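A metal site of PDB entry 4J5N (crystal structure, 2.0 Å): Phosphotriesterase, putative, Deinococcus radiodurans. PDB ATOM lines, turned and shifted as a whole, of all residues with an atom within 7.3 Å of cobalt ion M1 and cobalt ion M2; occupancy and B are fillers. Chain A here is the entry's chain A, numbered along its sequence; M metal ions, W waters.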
ATOM      1  N   HIS A  21     -18.803   8.779  26.996  1.00  0.00           N
ATOM      2  CA  HIS A  21     -17.994   9.988  27.167  1.00  0.00           C
ATOM      3  C   HIS A  21     -16.714   9.703  27.987  1.00  0.00           C
ATOM      4  O   HIS A  21     -16.770   9.670  29.215  1.00  0.00           O
ATOM      5  CB  HIS A  21     -18.824  11.074  27.874  1.00  0.00           C
ATOM      6  CG  HIS A  21     -18.250  12.452  27.811  1.00  0.00           C
ATOM      7  ND1 HIS A  21     -18.946  13.523  27.293  1.00  0.00           N
ATOM      8  CD2 HIS A  21     -17.056  12.956  28.213  1.00  0.00           C
ATOM      9  CE1 HIS A  21     -18.223  14.613  27.378  1.00  0.00           C
ATOM     10  NE2 HIS A  21     -17.060  14.292  27.938  1.00  0.00           N
ATOM     11  N   GLU A  22     -15.591   9.520  27.297  1.00  0.00           N
ATOM     12  CA  GLU A  22     -14.289   9.289  27.938  1.00  0.00           C
ATOM     13  C   GLU A  22     -13.217   9.988  27.106  1.00  0.00           C
ATOM     14  O   GLU A  22     -13.510  10.476  26.008  1.00  0.00           O
ATOM     15  CB  GLU A  22     -13.926   7.790  28.008  1.00  0.00           C
ATOM     16  CG  GLU A  22     -14.924   6.839  28.685  1.00  0.00           C
ATOM     17  CD  GLU A  22     -15.230   7.155  30.145  1.00  0.00           C
ATOM     18  OE1 GLU A  22     -14.366   7.705  30.860  1.00  0.00           O
ATOM     19  OE2 GLU A  22     -16.358   6.844  30.595  1.00  0.00           O
ATOM     20  N   HIS A  23     -12.003  10.089  27.640  1.00  0.00           N
ATOM     21  CA  HIS A  23     -10.887  10.708  26.909  1.00  0.00           C
ATOM     22  C   HIS A  23      -9.651   9.828  27.018  1.00  0.00           C
ATOM     23  O   HIS A  23      -9.099   9.685  28.107  1.00  0.00           O
ATOM     24  CB  HIS A  23     -10.553  12.099  27.469  1.00  0.00           C
ATOM     25  CG  HIS A  23     -11.711  13.053  27.486  1.00  0.00           C
ATOM     26  ND1 HIS A  23     -12.125  13.744  26.363  1.00  0.00           N
ATOM     27  CD2 HIS A  23     -12.563  13.400  28.477  1.00  0.00           C
ATOM     28  CE1 HIS A  23     -13.183  14.469  26.672  1.00  0.00           C
ATOM     29  NE2 HIS A  23     -13.467  14.274  27.942  1.00  0.00           N
ATOM     30  N   PHE A  26      -6.111  13.704  26.702  1.00  0.00           N
ATOM     31  CA  PHE A  26      -6.720  15.024  26.857  1.00  0.00           C
ATOM     32  C   PHE A  26      -5.699  16.012  27.369  1.00  0.00           C
ATOM     33  O   PHE A  26      -4.919  15.732  28.305  1.00  0.00           O
ATOM     34  CB  PHE A  26      -7.917  14.966  27.833  1.00  0.00           C
ATOM     35  CG  PHE A  26      -8.764  16.231  27.899  1.00  0.00           C
ATOM     36  CD1 PHE A  26      -8.461  17.269  28.820  1.00  0.00           C
ATOM     37  CD2 PHE A  26      -9.909  16.364  27.091  1.00  0.00           C
ATOM     38  CE1 PHE A  26      -9.299  18.413  28.937  1.00  0.00           C
ATOM     39  CE2 PHE A  26     -10.758  17.510  27.190  1.00  0.00           C
ATOM     40  CZ  PHE A  26     -10.454  18.535  28.113  1.00  0.00           C
ATOM     41  N   ALA A  67     -14.748  11.752  23.581  1.00  0.00           N
ATOM     42  CA  ALA A  67     -15.366  13.061  23.450  1.00  0.00           C
ATOM     43  C   ALA A  67     -14.435  14.249  23.332  1.00  0.00           C
ATOM     44  O   ALA A  67     -14.905  15.393  23.399  1.00  0.00           O
ATOM     45  CB  ALA A  67     -16.300  13.262  24.596  1.00  0.00           C
ATOM     46  N   THR A  68     -13.150  13.984  23.123  1.00  0.00           N
ATOM     47  CA  THR A  68     -12.125  15.030  23.034  1.00  0.00           C
ATOM     48  C   THR A  68     -12.293  16.050  21.896  1.00  0.00           C
ATOM     49  O   THR A  68     -12.263  15.675  20.718  1.00  0.00           O
ATOM     50  CB  THR A  68     -10.683  14.406  22.974  1.00  0.00           C
ATOM     51  OG1 THR A  68     -10.588  13.383  23.971  1.00  0.00           O
ATOM     52  CG2 THR A  68      -9.624  15.456  23.250  1.00  0.00           C
ATOM     53  N   PRO A  69     -12.480  17.342  22.244  1.00  0.00           N
ATOM     54  CA  PRO A  69     -12.644  18.423  21.260  1.00  0.00           C
ATOM     55  C   PRO A  69     -11.351  18.655  20.482  1.00  0.00           C
ATOM     56  O   PRO A  69     -10.260  18.359  20.989  1.00  0.00           O
ATOM     57  CB  PRO A  69     -12.972  19.634  22.136  1.00  0.00           C
ATOM     58  CG  PRO A  69     -13.665  19.022  23.323  1.00  0.00           C
ATOM     59  CD  PRO A  69     -12.784  17.844  23.597  1.00  0.00           C
ATOM     60  N   TYR A  97     -14.296  23.161  22.356  1.00  0.00           N
ATOM     61  CA  TYR A  97     -14.683  23.247  23.760  1.00  0.00           C
ATOM     62  C   TYR A  97     -15.434  24.572  24.034  1.00  0.00           C
ATOM     63  O   TYR A  97     -15.554  25.412  23.138  1.00  0.00           O
ATOM     64  CB  TYR A  97     -13.417  23.134  24.633  1.00  0.00           C
ATOM     65  CG  TYR A  97     -13.554  22.459  25.984  1.00  0.00           C
ATOM     66  CD1 TYR A  97     -14.457  21.398  26.197  1.00  0.00           C
ATOM     67  CD2 TYR A  97     -12.705  22.838  27.054  1.00  0.00           C
ATOM     68  CE1 TYR A  97     -14.517  20.712  27.451  1.00  0.00           C
ATOM     69  CE2 TYR A  97     -12.758  22.161  28.316  1.00  0.00           C
ATOM     70  CZ  TYR A  97     -13.667  21.095  28.501  1.00  0.00           C
ATOM     71  OH  TYR A  97     -13.727  20.429  29.700  1.00  0.00           O
ATOM     72  N   TYR A  98     -15.918  24.756  25.273  1.00  0.00           N
ATOM     73  CA  TYR A  98     -16.659  25.976  25.648  1.00  0.00           C
ATOM     74  C   TYR A  98     -15.779  27.250  25.669  1.00  0.00           C
ATOM     75  O   TYR A  98     -14.558  27.163  25.729  1.00  0.00           O
ATOM     76  CB  TYR A  98     -17.447  25.768  26.965  1.00  0.00           C
ATOM     77  CG  TYR A  98     -16.657  25.705  28.263  1.00  0.00           C
ATOM     78  CD1 TYR A  98     -15.711  24.676  28.507  1.00  0.00           C
ATOM     79  CD2 TYR A  98     -16.829  26.703  29.252  1.00  0.00           C
ATOM     80  CE1 TYR A  98     -14.945  24.653  29.709  1.00  0.00           C
ATOM     81  CE2 TYR A  98     -16.071  26.686  30.454  1.00  0.00           C
ATOM     82  CZ  TYR A  98     -15.131  25.667  30.677  1.00  0.00           C
ATOM     83  OH  TYR A  98     -14.366  25.678  31.821  1.00  0.00           O
ATOM     84  N   KCX A 143     -19.078  16.977  19.049  1.00  0.00           N
ATOM     85  CA  KCX A 143     -19.010  17.415  20.446  1.00  0.00           C
ATOM     86  CB  KCX A 143     -17.596  17.155  20.987  1.00  0.00           C
ATOM     87  CG  KCX A 143     -17.373  17.708  22.385  1.00  0.00           C
ATOM     88  CD  KCX A 143     -18.331  17.092  23.417  1.00  0.00           C
ATOM     89  CE  KCX A 143     -17.996  17.576  24.826  1.00  0.00           C
ATOM     90  NZ  KCX A 143     -16.655  17.103  25.224  1.00  0.00           N
ATOM     91  C   KCX A 143     -19.329  18.912  20.513  1.00  0.00           C
ATOM     92  O   KCX A 143     -18.725  19.720  19.824  1.00  0.00           O
ATOM     93  CX  KCX A 143     -16.227  17.149  26.478  1.00  0.00           C
ATOM     94  OQ1 KCX A 143     -16.991  17.614  27.357  1.00  0.00           O
ATOM     95  OQ2 KCX A 143     -15.082  16.711  26.720  1.00  0.00           O
ATOM     96  N   LEU A 144     -20.289  19.259  21.369  1.00  0.00           N
ATOM     97  CA  LEU A 144     -20.695  20.638  21.588  1.00  0.00           C
ATOM     98  C   LEU A 144     -20.522  20.963  23.047  1.00  0.00           C
ATOM     99  O   LEU A 144     -20.633  20.091  23.901  1.00  0.00           O
ATOM    100  CB  LEU A 144     -22.165  20.834  21.193  1.00  0.00           C
ATOM    101  CG  LEU A 144     -22.542  20.704  19.727  1.00  0.00           C
ATOM    102  CD1 LEU A 144     -24.029  20.848  19.573  1.00  0.00           C
ATOM    103  CD2 LEU A 144     -21.804  21.755  18.906  1.00  0.00           C
ATOM    104  N   ALA A 145     -20.259  22.230  23.343  1.00  0.00           N
ATOM    105  CA  ALA A 145     -20.073  22.673  24.717  1.00  0.00           C
ATOM    106  C   ALA A 145     -20.634  24.066  24.931  1.00  0.00           C
ATOM    107  O   ALA A 145     -20.610  24.895  24.020  1.00  0.00           O
ATOM    108  CB  ALA A 145     -18.604  22.641  25.050  1.00  0.00           C
ATOM    109  N   THR A 175     -22.768  16.367  24.166  1.00  0.00           N
ATOM    110  CA  THR A 175     -22.429  17.686  24.677  1.00  0.00           C
ATOM    111  C   THR A 175     -21.757  17.743  26.058  1.00  0.00           C
ATOM    112  O   THR A 175     -21.710  16.756  26.778  1.00  0.00           O
ATOM    113  CB  THR A 175     -23.677  18.636  24.753  1.00  0.00           C
ATOM    114  OG1 THR A 175     -24.395  18.363  25.956  1.00  0.00           O
ATOM    115  CG2 THR A 175     -24.609  18.497  23.541  1.00  0.00           C
ATOM    116  N   HIS A 176     -21.332  18.954  26.406  1.00  0.00           N
ATOM    117  CA  HIS A 176     -20.728  19.304  27.685  1.00  0.00           C
ATOM    118  C   HIS A 176     -21.620  20.417  28.253  1.00  0.00           C
ATOM    119  O   HIS A 176     -21.990  21.333  27.514  1.00  0.00           O
ATOM    120  CB  HIS A 176     -19.268  19.811  27.455  1.00  0.00           C
ATOM    121  CG  HIS A 176     -18.708  20.696  28.551  1.00  0.00           C
ATOM    122  ND1 HIS A 176     -17.850  20.223  29.518  1.00  0.00           N
ATOM    123  CD2 HIS A 176     -18.875  22.020  28.806  1.00  0.00           C
ATOM    124  CE1 HIS A 176     -17.506  21.206  30.327  1.00  0.00           C
ATOM    125  NE2 HIS A 176     -18.117  22.315  29.921  1.00  0.00           N
ATOM    126  N   THR A 177     -21.953  20.319  29.545  1.00  0.00           N
ATOM    127  CA  THR A 177     -22.687  21.366  30.240  1.00  0.00           C
ATOM    128  C   THR A 177     -21.775  21.789  31.394  1.00  0.00           C
ATOM    129  O   THR A 177     -21.147  20.946  32.048  1.00  0.00           O
ATOM    130  CB  THR A 177     -24.074  20.930  30.815  1.00  0.00           C
ATOM    131  OG1 THR A 177     -23.959  19.736  31.580  1.00  0.00           O
ATOM    132  CG2 THR A 177     -25.084  20.736  29.689  1.00  0.00           C
ATOM    133  N   GLN A 178     -21.661  23.101  31.597  1.00  0.00           N
ATOM    134  CA  GLN A 178     -20.805  23.638  32.648  1.00  0.00           C
ATOM    135  C   GLN A 178     -21.565  23.920  33.933  1.00  0.00           C
ATOM    136  O   GLN A 178     -22.618  24.574  33.923  1.00  0.00           O
ATOM    137  CB  GLN A 178     -20.098  24.904  32.125  1.00  0.00           C
ATOM    138  CG  GLN A 178     -19.054  25.541  33.049  1.00  0.00           C
ATOM    139  CD  GLN A 178     -17.792  24.691  33.230  1.00  0.00           C
ATOM    140  OE1 GLN A 178     -17.450  23.868  32.374  1.00  0.00           O
ATOM    141  NE2 GLN A 178     -17.093  24.911  34.339  1.00  0.00           N
ATOM    142  N   GLY A 203     -24.676  16.065  27.869  1.00  0.00           N
ATOM    143  CA  GLY A 203     -23.729  15.604  28.878  1.00  0.00           C
ATOM    144  C   GLY A 203     -23.632  16.409  30.150  1.00  0.00           C
ATOM    145  O   GLY A 203     -24.239  17.475  30.258  1.00  0.00           O
ATOM    146  N   HIS A 204     -22.827  15.887  31.084  1.00  0.00           N
ATOM    147  CA  HIS A 204     -22.560  16.450  32.420  1.00  0.00           C
ATOM    148  C   HIS A 204     -23.821  16.792  33.190  1.00  0.00           C
ATOM    149  O   HIS A 204     -23.845  17.695  34.043  1.00  0.00           O
ATOM    150  CB  HIS A 204     -21.578  17.634  32.365  1.00  0.00           C
ATOM    151  CG  HIS A 204     -20.305  17.354  31.613  1.00  0.00           C
ATOM    152  ND1 HIS A 204     -19.906  16.089  31.250  1.00  0.00           N
ATOM    153  CD2 HIS A 204     -19.376  18.192  31.104  1.00  0.00           C
ATOM    154  CE1 HIS A 204     -18.800  16.161  30.538  1.00  0.00           C
ATOM    155  NE2 HIS A 204     -18.455  17.428  30.436  1.00  0.00           N
ATOM    156  N   ASP A 227     -22.385  11.477  33.080  1.00  0.00           N
ATOM    157  CA  ASP A 227     -21.066  11.162  32.563  1.00  0.00           C
ATOM    158  C   ASP A 227     -19.777  11.540  33.280  1.00  0.00           C
ATOM    159  O   ASP A 227     -18.707  11.430  32.680  1.00  0.00           O
ATOM    160  CB  ASP A 227     -20.999  11.531  31.075  1.00  0.00           C
ATOM    161  CG  ASP A 227     -21.193  13.014  30.799  1.00  0.00           C
ATOM    162  OD1 ASP A 227     -21.028  13.812  31.739  1.00  0.00           O
ATOM    163  OD2 ASP A 227     -21.524  13.375  29.659  1.00  0.00           O
ATOM    164  N   ARG A 228     -19.852  12.032  34.508  1.00  0.00           N
ATOM    165  CA  ARG A 228     -18.652  12.377  35.269  1.00  0.00           C
ATOM    166  C   ARG A 228     -18.654  11.536  36.551  1.00  0.00           C
ATOM    167  O   ARG A 228     -18.202  11.981  37.604  1.00  0.00           O
ATOM    168  CB  ARG A 228     -18.566  13.889  35.576  1.00  0.00           C
ATOM    169  CG  ARG A 228     -18.808  14.802  34.379  1.00  0.00           C
ATOM    170  CD  ARG A 228     -18.386  16.225  34.647  1.00  0.00           C
ATOM    171  NE  ARG A 228     -16.964  16.410  34.422  1.00  0.00           N
ATOM    172  CZ  ARG A 228     -16.319  17.575  34.550  1.00  0.00           C
ATOM    173  NH1 ARG A 228     -16.979  18.672  34.901  1.00  0.00           N
ATOM    174  NH2 ARG A 228     -15.014  17.642  34.328  1.00  0.00           N
ATOM    175  N   HIS A 263     -17.664   8.113  32.714  1.00  0.00           N
ATOM    176  CA  HIS A 263     -16.808   8.698  33.756  1.00  0.00           C
ATOM    177  C   HIS A 263     -16.159  10.025  33.440  1.00  0.00           C
ATOM    178  O   HIS A 263     -15.801  10.762  34.364  1.00  0.00           O
ATOM    179  CB  HIS A 263     -15.653   7.748  34.132  1.00  0.00           C
ATOM    180  CG  HIS A 263     -16.066   6.325  34.317  1.00  0.00           C
ATOM    181  ND1 HIS A 263     -16.142   5.436  33.274  1.00  0.00           N
ATOM    182  CD2 HIS A 263     -16.411   5.641  35.430  1.00  0.00           C
ATOM    183  CE1 HIS A 263     -16.514   4.257  33.737  1.00  0.00           C
ATOM    184  NE2 HIS A 263     -16.683   4.351  35.046  1.00  0.00           N
ATOM    185  N   ASP A 264     -15.988  10.337  32.139  1.00  0.00           N
ATOM    186  CA  ASP A 264     -15.304  11.557  31.660  1.00  0.00           C
ATOM    187  C   ASP A 264     -13.836  11.498  32.143  1.00  0.00           C
ATOM    188  O   ASP A 264     -13.211  12.530  32.455  1.00  0.00           O
ATOM    189  CB  ASP A 264     -16.010  12.862  32.136  1.00  0.00           C
ATOM    190  CG  ASP A 264     -15.513  14.102  31.399  1.00  0.00           C
ATOM    191  OD1 ASP A 264     -14.906  13.968  30.324  1.00  0.00           O
ATOM    192  OD2 ASP A 264     -15.710  15.226  31.925  1.00  0.00           O
ATOM    193  N   SER A 265     -13.311  10.270  32.184  1.00  0.00           N
ATOM    194  CA  SER A 265     -11.939   9.995  32.622  1.00  0.00           C
ATOM    195  C   SER A 265     -10.916  10.371  31.570  1.00  0.00           C
ATOM    196  O   SER A 265     -11.231  10.480  30.379  1.00  0.00           O
ATOM    197  CB  SER A 265     -11.783   8.509  32.958  1.00  0.00           C
ATOM    198  OG  SER A 265     -11.836   7.705  31.791  1.00  0.00           O
ATOM    199  N   ILE A 266      -9.695  10.598  32.028  1.00  0.00           N
ATOM    200  CA  ILE A 266      -8.581  10.948  31.149  1.00  0.00           C
ATOM    201  C   ILE A 266      -7.536   9.866  31.425  1.00  0.00           C
ATOM    202  O   ILE A 266      -7.026   9.765  32.546  1.00  0.00           O
ATOM    203  CB  ILE A 266      -8.074  12.381  31.451  1.00  0.00           C
ATOM    204  CG1 ILE A 266      -9.188  13.396  31.128  1.00  0.00           C
ATOM    205  CG2 ILE A 266      -6.827  12.689  30.596  1.00  0.00           C
ATOM    206  CD1 ILE A 266      -9.042  14.755  31.741  1.00  0.00           C
HETATM  207 CO    CO M   1     -16.884  18.305  29.373  1.00  0.00          CO
HETATM  208 CO    CO M   2     -15.106  15.294  28.537  1.00  0.00          CO
HETATM  209  O   HOH W   1     -16.011  18.871  31.615  1.00  0.00           O
HETATM  210  O   HOH W   2     -15.453  16.527  29.712  1.00  0.00           O
HETATM  211  O   HOH W   3     -13.028  17.226  29.986  1.00  0.00           O
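Tyr 97 touches cobalt ion M1.
Within 4 Å of cobalt ion M1: Tyr 97, KCX 143, His 176 and His 204.
Cobalt ion M1 is bound by a ring nitrogen (NE2) of His 204 (2.1 Å), OQ1 of KCX 143 (2.1 Å), a ring nitrogen (ND1) of His 176 (2.2 Å), water W2 (2.3 Å) and water W1 (2.5 Å).
Cobalt ion M1 has five donor atoms within binding distance.
A ring nitrogen (ND1) of His 23 sits at hydrogen-bond distance from the side-chain hydroxyl (OG1) of Thr 68 (2.9 Å).
The side-chain carboxylate (OD1) of Asp 227 sits at hydrogen-bond distance from a ring nitrogen (ND1) of His 204 (2.6 Å).
NZ of KCX 143 is in hydrogen-bond range of the backbone carbonyl oxygen (O) of Ala 67 (3.1 Å).
NE2 of His 176 sits at hydrogen-bond distance from OE1 of Gln 178, 3.0 Å away.
O of Leu 144 sits at hydrogen-bond distance from N of His 176 (2.8 Å).
OD2 of Asp 264 is in salt-bridge range of NE of Arg 228 (3.0 Å).
The backbone NH of Asp 264 lies within hydrogen-bond range of the side-chain carboxylate of Glu 22, 3.3 Å away.
The backbone NH of Asp 264 is in hydrogen-bond range of the backbone carbonyl oxygen of Asp 227 (3.0 Å).
The nearest printed residue that does not touch cobalt ion M2 is His 204 (4.3 Å).
Cobalt ion M2 is bound by water W2 (1.7 Å), a ring nitrogen (NE2) of His 23 (2.0 Å), the side-chain carboxylate (OD1) of Asp 264 (2.2 Å), a ring nitrogen (NE2) of His 21 (2.3 Å) and OQ2 of KCX 143 (2.3 Å).
Cobalt ion M2 has five donor atoms within binding distance.
Water W1 lies within hydrogen-bond range of the guanidinium group of Arg 228 (3.1 Å) and the side-chain hydroxyl of Tyr 97 (3.4 Å).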
